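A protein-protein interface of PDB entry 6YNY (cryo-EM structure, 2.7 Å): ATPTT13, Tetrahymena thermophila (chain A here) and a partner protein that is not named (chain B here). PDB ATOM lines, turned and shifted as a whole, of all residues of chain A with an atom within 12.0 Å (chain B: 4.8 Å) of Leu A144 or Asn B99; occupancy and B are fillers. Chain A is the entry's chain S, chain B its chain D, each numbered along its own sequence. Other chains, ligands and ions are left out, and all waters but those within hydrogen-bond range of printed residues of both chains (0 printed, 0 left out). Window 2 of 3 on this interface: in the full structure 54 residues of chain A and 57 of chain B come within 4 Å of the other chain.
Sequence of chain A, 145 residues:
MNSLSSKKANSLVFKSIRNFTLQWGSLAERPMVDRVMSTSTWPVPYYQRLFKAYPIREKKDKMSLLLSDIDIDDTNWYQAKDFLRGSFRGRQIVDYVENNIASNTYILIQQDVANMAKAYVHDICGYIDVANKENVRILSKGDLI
OD1 of Asn B99 sits close to O of Asp A143, 3.4 Å away. O of Leu A144 sits at hydrogen-bond distance from ND2 of Asn B99, at 3.0 Å.
OG of Ser B102 lies within hydrogen-bond range of O of Asn B99 (2.5 Å).
Leu B103 touches Ile A138. O of Gly A142 touches CD1 of Leu B103, at 3.98 Å. CA of Tyr B100 touches CD1 of Leu A144 (3.5 Å). Ile A145 touches Val B96 (O to CG2, 3.4 Å).
Of chain B, only Asn B99 (3.0 Å) and Tyr B100 (3.5 Å) come within 4 Å of Leu A144. No residue of chain A comes within 4 Å of Lys B95. No residue of chain A comes within 4 Å of Glu B98. No residue of chain A comes within 4 Å of Ser B102. Of the printed residues of chain A, Leu B103 touches Ile A138 and Gly A142. Of the printed residues of chain B, Ile A145 touches Val B96 (3.4 Å). Of the printed residues of chain B, Gly A142 touches Leu B103 (3.98 Å). Printed residues of chain B within 4 Å of Ile A138: Leu B103 (3.5 Å). Of the printed residues of chain B, Asp A143 touches Asn B99 (2.3 Å). Lys A141 touches none of the printed residues of chain B.
Of the 9 printed residues of chain B, 4 touch a printed residue of chain A. Printed residues of chain B that touch a printed residue of chain A: Val B96, Asn B99, Tyr B100 and Leu B103. Hydrophobic or aromatic side chains of chain B that line the printed part of chain A: Val B96, Tyr B100 and Leu B103. Of the 11 printed residues of chain A, 5 touch a printed residue of chain B.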
ATOM      1  N   ASN A 135       4.252 -15.036  -9.948  1.00  0.00           N
ATOM      2  CA  ASN A 135       2.799 -15.115 -10.041  1.00  0.00           C
ATOM      3  C   ASN A 135       2.333 -15.000 -11.485  1.00  0.00           C
ATOM      4  O   ASN A 135       1.338 -15.624 -11.869  1.00  0.00           O
ATOM      5  CB  ASN A 135       2.163 -14.021  -9.184  1.00  0.00           C
ATOM      6  CG  ASN A 135       2.572 -14.112  -7.728  1.00  0.00           C
ATOM      7  OD1 ASN A 135       2.818 -15.199  -7.208  1.00  0.00           O
ATOM      8  ND2 ASN A 135       2.650 -12.966  -7.063  1.00  0.00           N
ATOM      9  N   VAL A 136       3.037 -14.210 -12.298  1.00  0.00           N
ATOM     10  CA  VAL A 136       2.679 -14.078 -13.707  1.00  0.00           C
ATOM     11  C   VAL A 136       2.727 -15.437 -14.390  1.00  0.00           C
ATOM     12  O   VAL A 136       1.791 -15.832 -15.095  1.00  0.00           O
ATOM     13  CB  VAL A 136       3.608 -13.065 -14.402  1.00  0.00           C
ATOM     14  CG1 VAL A 136       3.421 -13.117 -15.907  1.00  0.00           C
ATOM     15  CG2 VAL A 136       3.345 -11.666 -13.883  1.00  0.00           C
ATOM     16  N   ARG A 137       3.817 -16.177 -14.188  1.00  0.00           N
ATOM     17  CA  ARG A 137       3.955 -17.480 -14.831  1.00  0.00           C
ATOM     18  C   ARG A 137       2.901 -18.455 -14.321  1.00  0.00           C
ATOM     19  O   ARG A 137       2.226 -19.125 -15.111  1.00  0.00           O
ATOM     20  CB  ARG A 137       5.356 -18.036 -14.584  1.00  0.00           C
ATOM     21  CG  ARG A 137       5.641 -19.338 -15.310  1.00  0.00           C
ATOM     22  CD  ARG A 137       7.053 -19.823 -15.040  1.00  0.00           C
ATOM     23  NE  ARG A 137       7.234 -20.211 -13.643  1.00  0.00           N
ATOM     24  CZ  ARG A 137       8.383 -20.630 -13.122  1.00  0.00           C
ATOM     25  NH1 ARG A 137       9.470 -20.718 -13.878  1.00  0.00           N
ATOM     26  NH2 ARG A 137       8.446 -20.962 -11.840  1.00  0.00           N
ATOM     27  N   ILE A 138       2.747 -18.548 -12.999  1.00  0.00           N
ATOM     28  CA  ILE A 138       1.802 -19.503 -12.426  1.00  0.00           C
ATOM     29  C   ILE A 138       0.377 -19.154 -12.835  1.00  0.00           C
ATOM     30  O   ILE A 138      -0.427 -20.038 -13.158  1.00  0.00           O
ATOM     31  CB  ILE A 138       1.954 -19.553 -10.895  1.00  0.00           C
ATOM     32  CG1 ILE A 138       3.356 -20.038 -10.520  1.00  0.00           C
ATOM     33  CG2 ILE A 138       0.890 -20.459 -10.288  1.00  0.00           C
ATOM     34  CD1 ILE A 138       3.662 -19.951  -9.042  1.00  0.00           C
ATOM     35  N   LEU A 139       0.038 -17.863 -12.830  1.00  0.00           N
ATOM     36  CA  LEU A 139      -1.328 -17.457 -13.143  1.00  0.00           C
ATOM     37  C   LEU A 139      -1.580 -17.442 -14.646  1.00  0.00           C
ATOM     38  O   LEU A 139      -2.684 -17.773 -15.092  1.00  0.00           O
ATOM     39  CB  LEU A 139      -1.611 -16.083 -12.539  1.00  0.00           C
ATOM     40  CG  LEU A 139      -1.557 -16.029 -11.010  1.00  0.00           C
ATOM     41  CD1 LEU A 139      -1.711 -14.602 -10.515  1.00  0.00           C
ATOM     42  CD2 LEU A 139      -2.626 -16.924 -10.401  1.00  0.00           C
ATOM     43  N   SER A 140      -0.578 -17.064 -15.441  1.00  0.00           N
ATOM     44  CA  SER A 140      -0.724 -17.128 -16.890  1.00  0.00           C
ATOM     45  C   SER A 140      -0.723 -18.560 -17.409  1.00  0.00           C
ATOM     46  O   SER A 140      -0.990 -18.769 -18.597  1.00  0.00           O
ATOM     47  CB  SER A 140       0.394 -16.336 -17.568  1.00  0.00           C
ATOM     48  OG  SER A 140       0.376 -14.980 -17.159  1.00  0.00           O
ATOM     49  N   LYS A 141      -0.426 -19.539 -16.554  1.00  0.00           N
ATOM     50  CA  LYS A 141      -0.441 -20.935 -16.977  1.00  0.00           C
ATOM     51  C   LYS A 141      -1.816 -21.330 -17.499  1.00  0.00           C
ATOM     52  O   LYS A 141      -1.970 -21.714 -18.664  1.00  0.00           O
ATOM     53  CB  LYS A 141      -0.027 -21.830 -15.806  1.00  0.00           C
ATOM     54  CG  LYS A 141       0.008 -23.320 -16.123  1.00  0.00           C
ATOM     55  CD  LYS A 141       0.957 -23.650 -17.269  1.00  0.00           C
ATOM     56  CE  LYS A 141       2.381 -23.190 -16.984  1.00  0.00           C
ATOM     57  NZ  LYS A 141       2.893 -23.704 -15.683  1.00  0.00           N
ATOM     58  N   GLY A 142      -2.832 -21.243 -16.642  1.00  0.00           N
ATOM     59  CA  GLY A 142      -4.183 -21.577 -17.034  1.00  0.00           C
ATOM     60  C   GLY A 142      -5.180 -20.633 -16.395  1.00  0.00           C
ATOM     61  O   GLY A 142      -4.888 -19.955 -15.408  1.00  0.00           O
ATOM     62  N   ASP A 143      -6.373 -20.601 -16.982  1.00  0.00           N
ATOM     63  CA  ASP A 143      -7.461 -19.758 -16.507  1.00  0.00           C
ATOM     64  C   ASP A 143      -8.422 -20.604 -15.684  1.00  0.00           C
ATOM     65  O   ASP A 143      -8.891 -21.649 -16.149  1.00  0.00           O
ATOM     66  CB  ASP A 143      -8.194 -19.103 -17.678  1.00  0.00           C
ATOM     67  CG  ASP A 143      -9.172 -18.036 -17.228  1.00  0.00           C
ATOM     68  OD1 ASP A 143      -9.247 -17.772 -16.011  1.00  0.00           O
ATOM     69  OD2 ASP A 143      -9.866 -17.461 -18.093  1.00  0.00           O
ATOM     70  N   LEU A 144      -8.709 -20.152 -14.462  1.00  0.00           N
ATOM     71  CA  LEU A 144      -9.565 -20.920 -13.564  1.00  0.00           C
ATOM     72  C   LEU A 144     -10.934 -21.168 -14.187  1.00  0.00           C
ATOM     73  O   LEU A 144     -11.314 -22.317 -14.443  1.00  0.00           O
ATOM     74  CB  LEU A 144      -9.704 -20.185 -12.230  1.00  0.00           C
ATOM     75  CG  LEU A 144     -10.481 -20.922 -11.138  1.00  0.00           C
ATOM     76  CD1 LEU A 144      -9.768 -22.207 -10.735  1.00  0.00           C
ATOM     77  CD2 LEU A 144     -10.689 -20.020  -9.935  1.00  0.00           C
ATOM     78  N   ILE A 145     -11.675 -20.095 -14.457  1.00  0.00           N
ATOM     79  CA  ILE A 145     -13.049 -20.163 -14.969  1.00  0.00           C
ATOM     80  C   ILE A 145     -13.789 -21.396 -14.460  1.00  0.00           C
ATOM     81  O   ILE A 145     -13.674 -21.760 -13.290  1.00  0.00           O
ATOM     82  CB  ILE A 145     -13.078 -20.112 -16.521  1.00  0.00           C
ATOM     83  CG1 ILE A 145     -12.221 -21.218 -17.154  1.00  0.00           C
ATOM     84  CG2 ILE A 145     -12.623 -18.746 -17.009  1.00  0.00           C
ATOM     85  CD1 ILE A 145     -12.853 -22.600 -17.130  1.00  0.00           C
ATOM     86  N   LYS B  95     -15.411 -28.920 -13.460  1.00  0.00           N
ATOM     87  CA  LYS B  95     -14.442 -28.172 -14.255  1.00  0.00           C
ATOM     88  C   LYS B  95     -13.669 -27.182 -13.393  1.00  0.00           C
ATOM     89  O   LYS B  95     -12.469 -26.970 -13.600  1.00  0.00           O
ATOM     90  CB  LYS B  95     -15.155 -27.447 -15.396  1.00  0.00           C
ATOM     91  CG  LYS B  95     -14.244 -26.585 -16.254  1.00  0.00           C
ATOM     92  CD  LYS B  95     -14.957 -26.087 -17.504  1.00  0.00           C
ATOM     93  CE  LYS B  95     -16.154 -25.211 -17.163  1.00  0.00           C
ATOM     94  NZ  LYS B  95     -16.813 -24.668 -18.382  1.00  0.00           N
ATOM     95  N   VAL B  96     -14.341 -26.561 -12.423  1.00  0.00           N
ATOM     96  CA  VAL B  96     -13.659 -25.638 -11.523  1.00  0.00           C
ATOM     97  C   VAL B  96     -12.677 -26.390 -10.635  1.00  0.00           C
ATOM     98  O   VAL B  96     -11.558 -25.924 -10.389  1.00  0.00           O
ATOM     99  CB  VAL B  96     -14.686 -24.852 -10.690  1.00  0.00           C
ATOM    100  CG1 VAL B  96     -13.986 -24.012  -9.635  1.00  0.00           C
ATOM    101  CG2 VAL B  96     -15.538 -23.974 -11.591  1.00  0.00           C
ATOM    102  N   LYS B  97     -13.074 -27.564 -10.141  1.00  0.00           N
ATOM    103  CA  LYS B  97     -12.206 -28.325  -9.248  1.00  0.00           C
ATOM    104  C   LYS B  97     -10.924 -28.743  -9.955  1.00  0.00           C
ATOM    105  O   LYS B  97      -9.818 -28.523  -9.447  1.00  0.00           O
ATOM    106  CB  LYS B  97     -12.952 -29.550  -8.718  1.00  0.00           C
ATOM    107  CG  LYS B  97     -12.153 -30.384  -7.731  1.00  0.00           C
ATOM    108  CD  LYS B  97     -12.976 -31.544  -7.195  1.00  0.00           C
ATOM    109  CE  LYS B  97     -12.162 -32.421  -6.257  1.00  0.00           C
ATOM    110  NZ  LYS B  97     -11.696 -31.680  -5.052  1.00  0.00           N
ATOM    111  N   GLU B  98     -11.050 -29.356 -11.136  1.00  0.00           N
ATOM    112  CA  GLU B  98      -9.867 -29.830 -11.845  1.00  0.00           C
ATOM    113  C   GLU B  98      -8.956 -28.673 -12.234  1.00  0.00           C
ATOM    114  O   GLU B  98      -7.727 -28.791 -12.163  1.00  0.00           O
ATOM    115  CB  GLU B  98     -10.283 -30.632 -13.080  1.00  0.00           C
ATOM    116  CG  GLU B  98     -11.113 -29.859 -14.100  1.00  0.00           C
ATOM    117  CD  GLU B  98     -10.268 -29.059 -15.077  1.00  0.00           C
ATOM    118  OE1 GLU B  98      -9.032 -29.237 -15.089  1.00  0.00           O
ATOM    119  OE2 GLU B  98     -10.843 -28.248 -15.834  1.00  0.00           O
ATOM    120  N   ASN B  99      -9.537 -27.544 -12.646  1.00  0.00           N
ATOM    121  CA  ASN B  99      -8.721 -26.384 -12.990  1.00  0.00           C
ATOM    122  C   ASN B  99      -8.160 -25.720 -11.738  1.00  0.00           C
ATOM    123  O   ASN B  99      -7.013 -25.259 -11.735  1.00  0.00           O
ATOM    124  CB  ASN B  99      -9.545 -25.389 -13.806  1.00  0.00           C
ATOM    125  CG  ASN B  99      -8.690 -24.317 -14.454  1.00  0.00           C
ATOM    126  OD1 ASN B  99      -7.687 -23.879 -13.891  1.00  0.00           O
ATOM    127  ND2 ASN B  99      -9.083 -23.891 -15.647  1.00  0.00           N
ATOM    128  N   TYR B 100      -8.955 -25.663 -10.669  1.00  0.00           N
ATOM    129  CA  TYR B 100      -8.462 -25.121  -9.408  1.00  0.00           C
ATOM    130  C   TYR B 100      -7.271 -25.924  -8.899  1.00  0.00           C
ATOM    131  O   TYR B 100      -6.224 -25.361  -8.563  1.00  0.00           O
ATOM    132  CB  TYR B 100      -9.590 -25.113  -8.375  1.00  0.00           C
ATOM    133  CG  TYR B 100      -9.123 -24.980  -6.943  1.00  0.00           C
ATOM    134  CD1 TYR B 100      -8.871 -23.734  -6.388  1.00  0.00           C
ATOM    135  CD2 TYR B 100      -8.947 -26.102  -6.145  1.00  0.00           C
ATOM    136  CE1 TYR B 100      -8.447 -23.610  -5.079  1.00  0.00           C
ATOM    137  CE2 TYR B 100      -8.524 -25.988  -4.835  1.00  0.00           C
ATOM    138  CZ  TYR B 100      -8.276 -24.739  -4.307  1.00  0.00           C
ATOM    139  OH  TYR B 100      -7.855 -24.621  -3.002  1.00  0.00           O
ATOM    140  N   GLU B 101      -7.415 -27.250  -8.847  1.00  0.00           N
ATOM    141  CA  GLU B 101      -6.349 -28.090  -8.313  1.00  0.00           C
ATOM    142  C   GLU B 101      -5.064 -27.950  -9.120  1.00  0.00           C
ATOM    143  O   GLU B 101      -3.968 -28.038  -8.558  1.00  0.00           O
ATOM    144  CB  GLU B 101      -6.802 -29.551  -8.286  1.00  0.00           C
ATOM    145  CG  GLU B 101      -5.805 -30.506  -7.644  1.00  0.00           C
ATOM    146  CD  GLU B 101      -5.611 -30.240  -6.164  1.00  0.00           C
ATOM    147  OE1 GLU B 101      -6.394 -29.454  -5.591  1.00  0.00           O
ATOM    148  OE2 GLU B 101      -4.675 -30.820  -5.573  1.00  0.00           O
ATOM    149  N   SER B 102      -5.178 -27.731 -10.432  1.00  0.00           N
ATOM    150  CA  SER B 102      -3.987 -27.652 -11.271  1.00  0.00           C
ATOM    151  C   SER B 102      -3.082 -26.504 -10.842  1.00  0.00           C
ATOM    152  O   SER B 102      -1.857 -26.655 -10.790  1.00  0.00           O
ATOM    153  CB  SER B 102      -4.390 -27.493 -12.736  1.00  0.00           C
ATOM    154  OG  SER B 102      -5.080 -26.273 -12.943  1.00  0.00           O
ATOM    155  N   LEU B 103      -3.666 -25.346 -10.530  1.00  0.00           N
ATOM    156  CA  LEU B 103      -2.860 -24.198 -10.134  1.00  0.00           C
ATOM    157  C   LEU B 103      -2.333 -24.339  -8.712  1.00  0.00           C
ATOM    158  O   LEU B 103      -1.269 -23.796  -8.395  1.00  0.00           O
ATOM    159  CB  LEU B 103      -3.673 -22.910 -10.267  1.00  0.00           C
ATOM    160  CG  LEU B 103      -4.134 -22.562 -11.684  1.00  0.00           C
ATOM    161  CD1 LEU B 103      -5.001 -21.315 -11.669  1.00  0.00           C
ATOM    162  CD2 LEU B 103      -2.945 -22.375 -12.614  1.00  0.00           C
